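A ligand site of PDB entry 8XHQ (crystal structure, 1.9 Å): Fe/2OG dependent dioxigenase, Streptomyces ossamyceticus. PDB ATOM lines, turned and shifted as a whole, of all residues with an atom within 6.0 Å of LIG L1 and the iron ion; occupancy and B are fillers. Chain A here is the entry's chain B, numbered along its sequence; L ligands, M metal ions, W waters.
An oxygen (O5) of LIG L1 sits at hydrogen-bond distance from the side-chain hydroxyl of Tyr 156. The side-chain hydroxyl (OG) of Ser 242 is in hydrogen-bond range of an oxygen (O5) of LIG L1, at 2.8 Å. The guanidinium group (NH2) of Arg 240 lies within salt-bridge range of an oxygen (O4) of LIG L1. A nitrogen (N2) of LG2 L2 sits close to the side-chain carboxylate (OD1) of Asp 170 (3.1 Å).
An oxygen (O1) of LIG L1 lies close to a nitrogen (N2) of LG2 L2, at 3.0 Å.
The side-chain carboxylate (OD2) of Asp 170 is in hydrogen-bond range of the side-chain hydroxyl (OG1) of Thr 175. OD2 of Asp 170 sits at hydrogen-bond distance from ND2 of Asn 205. N of Tyr 156 lies within hydrogen-bond range of O of Arg 240 (3.0 Å). The backbone carbonyl oxygen (O) of Ser 242 is in hydrogen-bond range of the backbone NH (N) of Ser 154 (2.8 Å). N of Cys 165 is in hydrogen-bond range of O of Val 228 (3.0 Å).
Leu 177 touches LIG L1. CG2 of Ile 179 touches O4 of LIG L1, 3.4 Å away. Leu 184 touches LIG L1 (CD1 to O4, 3.7 Å). CG2 of Val 228 touches C5 of LIG L1, 3.4 Å away. CZ of Phe 246 touches O2 of LIG L1, at 3.5 Å. Hydrophobic or aromatic side chains that line LIG L1: Tyr 156, His 168, Leu 177, Ile 179, Leu 184, His 226, Val 228 and Phe 246. 11 residues have an atom within 4 Å of LIG L1: Tyr 156, His 168, Asp 170, Leu 177, Ile 179, Leu 184, His 226, Val 228, Arg 240, Ser 242 and Phe 246.
Three residues have an atom within 4 Å of the iron ion: His 168, Asp 170 and His 226. The nearest printed residue that does not touch the iron ion is Phe 246 (4.8 Å).
The iron ion is bound by NE2 of His 226, OD1 of Asp 170, O3 of LIG L1, NE2 of His 168, O1 of LIG L1 and water W2. The iron ion has six donor atoms within binding distance.
Water W1 lies within hydrogen-bond range of O2 of LIG L1 (2.8 Å), OG of Ser 154 (2.8 Å) and OG of Ser 242 (2.9 Å).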
ATOM      1  N   ALA A 152      31.857   5.010 -23.175  1.00  0.00           N
ATOM      2  CA  ALA A 152      30.642   5.387 -22.466  1.00  0.00           C
ATOM      3  C   ALA A 152      30.923   5.438 -20.964  1.00  0.00           C
ATOM      4  O   ALA A 152      31.610   4.567 -20.417  1.00  0.00           O
ATOM      5  CB  ALA A 152      29.486   4.421 -22.737  1.00  0.00           C
ATOM      6  N   SER A 154      28.385   5.704 -17.652  1.00  0.00           N
ATOM      7  CA  SER A 154      26.968   5.681 -17.286  1.00  0.00           C
ATOM      8  C   SER A 154      26.764   5.899 -15.797  1.00  0.00           C
ATOM      9  O   SER A 154      27.452   5.274 -14.972  1.00  0.00           O
ATOM     10  CB  SER A 154      26.327   4.358 -17.709  1.00  0.00           C
ATOM     11  OG  SER A 154      26.288   4.258 -19.114  1.00  0.00           O
ATOM     12  N   TYR A 156      23.478   5.571 -13.186  1.00  0.00           N
ATOM     13  CA  TYR A 156      22.092   5.132 -13.019  1.00  0.00           C
ATOM     14  C   TYR A 156      21.421   5.939 -11.927  1.00  0.00           C
ATOM     15  O   TYR A 156      21.691   5.735 -10.738  1.00  0.00           O
ATOM     16  CB  TYR A 156      22.055   3.636 -12.725  1.00  0.00           C
ATOM     17  CG  TYR A 156      22.580   2.884 -13.922  1.00  0.00           C
ATOM     18  CD1 TYR A 156      23.952   2.672 -14.105  1.00  0.00           C
ATOM     19  CD2 TYR A 156      21.701   2.460 -14.922  1.00  0.00           C
ATOM     20  CE1 TYR A 156      24.423   2.003 -15.257  1.00  0.00           C
ATOM     21  CE2 TYR A 156      22.163   1.796 -16.044  1.00  0.00           C
ATOM     22  CZ  TYR A 156      23.511   1.586 -16.221  1.00  0.00           C
ATOM     23  OH  TYR A 156      23.920   0.940 -17.361  1.00  0.00           O
ATOM     24  N   CYS A 165      18.703   0.504 -17.812  1.00  0.00           N
ATOM     25  CA  CYS A 165      19.200   0.689 -19.177  1.00  0.00           C
ATOM     26  C   CYS A 165      18.268  -0.040 -20.133  1.00  0.00           C
ATOM     27  O   CYS A 165      17.879  -1.172 -19.857  1.00  0.00           O
ATOM     28  CB  CYS A 165      20.634   0.124 -19.342  1.00  0.00           C
ATOM     29  SG  CYS A 165      21.454   0.470 -20.906  1.00  0.00           S
ATOM     30  N   HIS A 168      19.271  -3.960 -24.982  1.00  0.00           N
ATOM     31  CA  HIS A 168      19.889  -3.727 -26.290  1.00  0.00           C
ATOM     32  C   HIS A 168      20.933  -4.787 -26.566  1.00  0.00           C
ATOM     33  O   HIS A 168      21.415  -5.480 -25.664  1.00  0.00           O
ATOM     34  CB  HIS A 168      20.535  -2.336 -26.375  1.00  0.00           C
ATOM     35  CG  HIS A 168      21.626  -2.125 -25.369  1.00  0.00           C
ATOM     36  ND1 HIS A 168      21.373  -1.825 -24.053  1.00  0.00           N
ATOM     37  CD2 HIS A 168      22.973  -2.174 -25.494  1.00  0.00           C
ATOM     38  CE1 HIS A 168      22.507  -1.701 -23.399  1.00  0.00           C
ATOM     39  NE2 HIS A 168      23.494  -1.894 -24.259  1.00  0.00           N
ATOM     40  N   LYS A 169      21.285  -4.886 -27.841  1.00  0.00           N
ATOM     41  CA  LYS A 169      22.548  -5.453 -28.274  1.00  0.00           C
ATOM     42  C   LYS A 169      23.502  -4.321 -28.591  1.00  0.00           C
ATOM     43  O   LYS A 169      23.131  -3.356 -29.247  1.00  0.00           O
ATOM     44  CB  LYS A 169      22.373  -6.348 -29.510  1.00  0.00           C
ATOM     45  CG  LYS A 169      21.371  -7.510 -29.305  1.00  0.00           C
ATOM     46  CD  LYS A 169      21.257  -8.357 -30.612  1.00  0.00           C
ATOM     47  CE  LYS A 169      20.319  -9.558 -30.451  1.00  0.00           C
ATOM     48  NZ  LYS A 169      20.264 -10.382 -31.720  1.00  0.00           N
ATOM     49  N   ASP A 170      24.736  -4.422 -28.094  1.00  0.00           N
ATOM     50  CA  ASP A 170      25.747  -3.442 -28.479  1.00  0.00           C
ATOM     51  C   ASP A 170      25.862  -3.430 -30.005  1.00  0.00           C
ATOM     52  O   ASP A 170      25.520  -4.405 -30.669  1.00  0.00           O
ATOM     53  CB  ASP A 170      27.103  -3.780 -27.824  1.00  0.00           C
ATOM     54  CG  ASP A 170      27.065  -3.539 -26.304  1.00  0.00           C
ATOM     55  OD1 ASP A 170      26.120  -2.882 -25.866  1.00  0.00           O
ATOM     56  OD2 ASP A 170      27.944  -4.002 -25.582  1.00  0.00           O
ATOM     57  N   THR A 175      32.975  -5.135 -27.075  1.00  0.00           N
ATOM     58  CA  THR A 175      32.792  -4.247 -25.931  1.00  0.00           C
ATOM     59  C   THR A 175      33.693  -4.706 -24.786  1.00  0.00           C
ATOM     60  O   THR A 175      33.778  -5.902 -24.510  1.00  0.00           O
ATOM     61  CB  THR A 175      31.335  -4.276 -25.449  1.00  0.00           C
ATOM     62  OG1 THR A 175      30.453  -3.956 -26.534  1.00  0.00           O
ATOM     63  CG2 THR A 175      31.133  -3.304 -24.272  1.00  0.00           C
ATOM     64  N   LEU A 177      33.787  -3.784 -20.819  1.00  0.00           N
ATOM     65  CA  LEU A 177      32.934  -3.072 -19.869  1.00  0.00           C
ATOM     66  C   LEU A 177      33.458  -3.225 -18.446  1.00  0.00           C
ATOM     67  O   LEU A 177      33.801  -4.335 -18.023  1.00  0.00           O
ATOM     68  CB  LEU A 177      31.496  -3.589 -19.948  1.00  0.00           C
ATOM     69  CG  LEU A 177      30.456  -3.186 -18.892  1.00  0.00           C
ATOM     70  CD1 LEU A 177      30.018  -1.728 -19.050  1.00  0.00           C
ATOM     71  CD2 LEU A 177      29.227  -4.120 -18.923  1.00  0.00           C
ATOM     72  N   ILE A 179      32.164  -2.966 -14.607  1.00  0.00           N
ATOM     73  CA  ILE A 179      31.077  -2.869 -13.642  1.00  0.00           C
ATOM     74  C   ILE A 179      31.578  -3.304 -12.269  1.00  0.00           C
ATOM     75  O   ILE A 179      32.505  -4.114 -12.146  1.00  0.00           O
ATOM     76  CB  ILE A 179      29.858  -3.741 -14.044  1.00  0.00           C
ATOM     77  CG1 ILE A 179      30.319  -5.180 -14.295  1.00  0.00           C
ATOM     78  CG2 ILE A 179      29.156  -3.131 -15.271  1.00  0.00           C
ATOM     79  CD1 ILE A 179      29.204  -6.211 -14.464  1.00  0.00           C
ATOM     80  N   GLY A 183      23.091  -5.822 -11.408  1.00  0.00           N
ATOM     81  CA  GLY A 183      22.094  -5.059 -12.129  1.00  0.00           C
ATOM     82  C   GLY A 183      22.086  -5.424 -13.600  1.00  0.00           C
ATOM     83  O   GLY A 183      21.031  -5.411 -14.241  1.00  0.00           O
ATOM     84  N   LEU A 184      23.243  -5.756 -14.136  1.00  0.00           N
ATOM     85  CA  LEU A 184      23.307  -6.194 -15.532  1.00  0.00           C
ATOM     86  C   LEU A 184      22.701  -7.587 -15.668  1.00  0.00           C
ATOM     87  O   LEU A 184      22.925  -8.461 -14.829  1.00  0.00           O
ATOM     88  CB  LEU A 184      24.758  -6.189 -16.009  1.00  0.00           C
ATOM     89  CG  LEU A 184      25.003  -6.622 -17.447  1.00  0.00           C
ATOM     90  CD1 LEU A 184      24.395  -5.634 -18.392  1.00  0.00           C
ATOM     91  CD2 LEU A 184      26.507  -6.754 -17.720  1.00  0.00           C
ATOM     92  N   ASN A 205      31.919  -8.470 -24.332  1.00  0.00           N
ATOM     93  CA  ASN A 205      30.944  -9.116 -25.209  1.00  0.00           C
ATOM     94  C   ASN A 205      31.105  -8.571 -26.610  1.00  0.00           C
ATOM     95  O   ASN A 205      31.961  -7.724 -26.890  1.00  0.00           O
ATOM     96  CB  ASN A 205      29.500  -8.935 -24.694  1.00  0.00           C
ATOM     97  CG  ASN A 205      29.111  -7.493 -24.552  1.00  0.00           C
ATOM     98  OD1 ASN A 205      29.264  -6.918 -23.487  1.00  0.00           O
ATOM     99  ND2 ASN A 205      28.608  -6.909 -25.625  1.00  0.00           N
ATOM    100  N   HIS A 226      21.073  -7.551 -23.569  1.00  0.00           N
ATOM    101  CA  HIS A 226      21.307  -7.291 -22.162  1.00  0.00           C
ATOM    102  C   HIS A 226      20.639  -5.993 -21.766  1.00  0.00           C
ATOM    103  O   HIS A 226      20.377  -5.110 -22.591  1.00  0.00           O
ATOM    104  CB  HIS A 226      22.811  -7.260 -21.839  1.00  0.00           C
ATOM    105  CG  HIS A 226      23.596  -6.316 -22.689  1.00  0.00           C
ATOM    106  ND1 HIS A 226      23.916  -6.586 -24.006  1.00  0.00           N
ATOM    107  CD2 HIS A 226      24.146  -5.116 -22.405  1.00  0.00           C
ATOM    108  CE1 HIS A 226      24.618  -5.577 -24.496  1.00  0.00           C
ATOM    109  NE2 HIS A 226      24.784  -4.680 -23.543  1.00  0.00           N
ATOM    110  N   ARG A 227      20.345  -5.891 -20.466  1.00  0.00           N
ATOM    111  CA  ARG A 227      19.752  -4.688 -19.905  1.00  0.00           C
ATOM    112  C   ARG A 227      20.343  -4.470 -18.520  1.00  0.00           C
ATOM    113  O   ARG A 227      21.018  -5.334 -17.974  1.00  0.00           O
ATOM    114  CB  ARG A 227      18.222  -4.801 -19.821  1.00  0.00           C
ATOM    115  CG  ARG A 227      17.762  -5.886 -18.863  1.00  0.00           C
ATOM    116  CD  ARG A 227      16.237  -5.887 -18.663  1.00  0.00           C
ATOM    117  NE  ARG A 227      15.865  -6.690 -17.505  1.00  0.00           N
ATOM    118  CZ  ARG A 227      14.627  -6.890 -17.081  1.00  0.00           C
ATOM    119  NH1 ARG A 227      14.408  -7.630 -15.991  1.00  0.00           N
ATOM    120  NH2 ARG A 227      13.596  -6.354 -17.740  1.00  0.00           N
ATOM    121  N   VAL A 228      20.033  -3.314 -17.936  1.00  0.00           N
ATOM    122  CA  VAL A 228      20.237  -3.086 -16.510  1.00  0.00           C
ATOM    123  C   VAL A 228      18.873  -2.901 -15.862  1.00  0.00           C
ATOM    124  O   VAL A 228      18.116  -1.989 -16.229  1.00  0.00           O
ATOM    125  CB  VAL A 228      21.152  -1.874 -16.246  1.00  0.00           C
ATOM    126  CG1 VAL A 228      21.338  -1.692 -14.750  1.00  0.00           C
ATOM    127  CG2 VAL A 228      22.514  -2.110 -16.915  1.00  0.00           C
ATOM    128  N   ARG A 240      24.707   3.156  -8.875  1.00  0.00           N
ATOM    129  CA  ARG A 240      25.358   2.295  -9.847  1.00  0.00           C
ATOM    130  C   ARG A 240      25.954   3.106 -10.974  1.00  0.00           C
ATOM    131  O   ARG A 240      25.381   4.102 -11.429  1.00  0.00           O
ATOM    132  CB  ARG A 240      24.375   1.272 -10.424  1.00  0.00           C
ATOM    133  CG  ARG A 240      25.083   0.193 -11.289  1.00  0.00           C
ATOM    134  CD  ARG A 240      24.123  -0.934 -11.662  1.00  0.00           C
ATOM    135  NE  ARG A 240      24.833  -2.069 -12.246  1.00  0.00           N
ATOM    136  CZ  ARG A 240      25.267  -2.095 -13.499  1.00  0.00           C
ATOM    137  NH1 ARG A 240      25.055  -1.037 -14.279  1.00  0.00           N
ATOM    138  NH2 ARG A 240      25.896  -3.171 -13.996  1.00  0.00           N
ATOM    139  N   PHE A 241      27.139   2.696 -11.425  1.00  0.00           N
ATOM    140  CA  PHE A 241      27.752   3.278 -12.603  1.00  0.00           C
ATOM    141  C   PHE A 241      28.383   2.161 -13.420  1.00  0.00           C
ATOM    142  O   PHE A 241      28.536   1.032 -12.949  1.00  0.00           O
ATOM    143  CB  PHE A 241      28.804   4.337 -12.233  1.00  0.00           C
ATOM    144  CG  PHE A 241      30.021   3.775 -11.528  1.00  0.00           C
ATOM    145  CD1 PHE A 241      31.081   3.272 -12.254  1.00  0.00           C
ATOM    146  CD2 PHE A 241      30.109   3.786 -10.139  1.00  0.00           C
ATOM    147  CE1 PHE A 241      32.198   2.764 -11.623  1.00  0.00           C
ATOM    148  CE2 PHE A 241      31.207   3.291  -9.489  1.00  0.00           C
ATOM    149  CZ  PHE A 241      32.274   2.771 -10.228  1.00  0.00           C
ATOM    150  N   SER A 242      28.765   2.483 -14.649  1.00  0.00           N
ATOM    151  CA  SER A 242      29.582   1.597 -15.463  1.00  0.00           C
ATOM    152  C   SER A 242      30.329   2.447 -16.475  1.00  0.00           C
ATOM    153  O   SER A 242      29.925   3.576 -16.773  1.00  0.00           O
ATOM    154  CB  SER A 242      28.733   0.526 -16.175  1.00  0.00           C
ATOM    155  OG  SER A 242      27.973   1.109 -17.244  1.00  0.00           O
ATOM    156  N   ALA A 244      32.779   1.827 -20.314  1.00  0.00           N
ATOM    157  CA  ALA A 244      33.069   0.826 -21.321  1.00  0.00           C
ATOM    158  C   ALA A 244      33.672   1.493 -22.537  1.00  0.00           C
ATOM    159  O   ALA A 244      33.443   2.676 -22.785  1.00  0.00           O
ATOM    160  CB  ALA A 244      31.785   0.069 -21.704  1.00  0.00           C
ATOM    161  N   PHE A 246      34.163   0.563 -26.844  1.00  0.00           N
ATOM    162  CA  PHE A 246      33.553  -0.239 -27.899  1.00  0.00           C
ATOM    163  C   PHE A 246      34.322   0.014 -29.190  1.00  0.00           C
ATOM    164  O   PHE A 246      34.589   1.164 -29.542  1.00  0.00           O
ATOM    165  CB  PHE A 246      32.073   0.104 -28.143  1.00  0.00           C
ATOM    166  CG  PHE A 246      31.239   0.331 -26.898  1.00  0.00           C
ATOM    167  CD1 PHE A 246      31.324   1.520 -26.188  1.00  0.00           C
ATOM    168  CD2 PHE A 246      30.289  -0.599 -26.510  1.00  0.00           C
ATOM    169  CE1 PHE A 246      30.529   1.734 -25.072  1.00  0.00           C
ATOM    170  CE2 PHE A 246      29.487  -0.398 -25.398  1.00  0.00           C
ATOM    171  CZ  PHE A 246      29.605   0.779 -24.683  1.00  0.00           C
HETATM  172  C1  LIG L   1      26.661  -0.328 -22.335  1.00  0.00           C
HETATM  173  O1  LIG L   1      26.460  -0.553 -23.541  1.00  0.00           O
HETATM  174  O2  LIG L   1      27.370   0.648 -21.997  1.00  0.00           O
HETATM  175  C2  LIG L   1      26.047  -1.174 -21.303  1.00  0.00           C
HETATM  176  O3  LIG L   1      25.331  -2.108 -21.573  1.00  0.00           O
HETATM  177  C3  LIG L   1      26.307  -0.957 -19.836  1.00  0.00           C
HETATM  178  C4  LIG L   1      25.591  -2.054 -19.021  1.00  0.00           C
HETATM  179  C5  LIG L   1      25.880  -1.799 -17.540  1.00  0.00           C
HETATM  180  O4  LIG L   1      26.165  -2.757 -16.807  1.00  0.00           O
HETATM  181  O5  LIG L   1      25.816  -0.629 -17.086  1.00  0.00           O
HETATM  182  C1  LG2 L   2      26.165   1.517 -28.617  1.00  0.00           C
HETATM  183  C2  LG2 L   2      26.522   0.300 -27.752  1.00  0.00           C
HETATM  184  C3  LG2 L   2      25.012   1.174 -25.875  1.00  0.00           C
HETATM  185  C4  LG2 L   2      24.236   1.904 -26.981  1.00  0.00           C
HETATM  186  C5  LG2 L   2      27.188   2.658 -28.447  1.00  0.00           C
HETATM  187  C6  LG2 L   2      28.603   2.166 -28.726  1.00  0.00           C
HETATM  188  C7  LG2 L   2      26.808   3.781 -29.450  1.00  0.00           C
HETATM  189  C8  LG2 L   2      26.844   3.312 -30.910  1.00  0.00           C
HETATM  190  C9  LG2 L   2      25.761   2.181 -24.968  1.00  0.00           C
HETATM  191  C10 LG2 L   2      24.763   2.950 -24.051  1.00  0.00           C
HETATM  192  C11 LG2 L   2      25.631   3.979 -23.290  1.00  0.00           C
HETATM  193  C12 LG2 L   2      24.082   2.014 -23.040  1.00  0.00           C
HETATM  194  N1  LG2 L   2      24.829   2.049 -28.312  1.00  0.00           N
HETATM  195  N2  LG2 L   2      25.942   0.179 -26.414  1.00  0.00           N
HETATM  196  O1  LG2 L   2      23.140   2.350 -26.775  1.00  0.00           O
HETATM  197  O2  LG2 L   2      27.258  -0.548 -28.149  1.00  0.00           O
HETATM  198  O3  LG2 L   2      25.617   2.719 -31.301  1.00  0.00           O
HETATM  199 FE    FE M   1      25.556  -2.609 -23.738  1.00  0.00          FE
HETATM  200  O   HOH W   1      28.168   2.253 -19.867  1.00  0.00           O
HETATM  201  O   HOH W   2      27.574  -3.496 -23.052  1.00  0.00           O
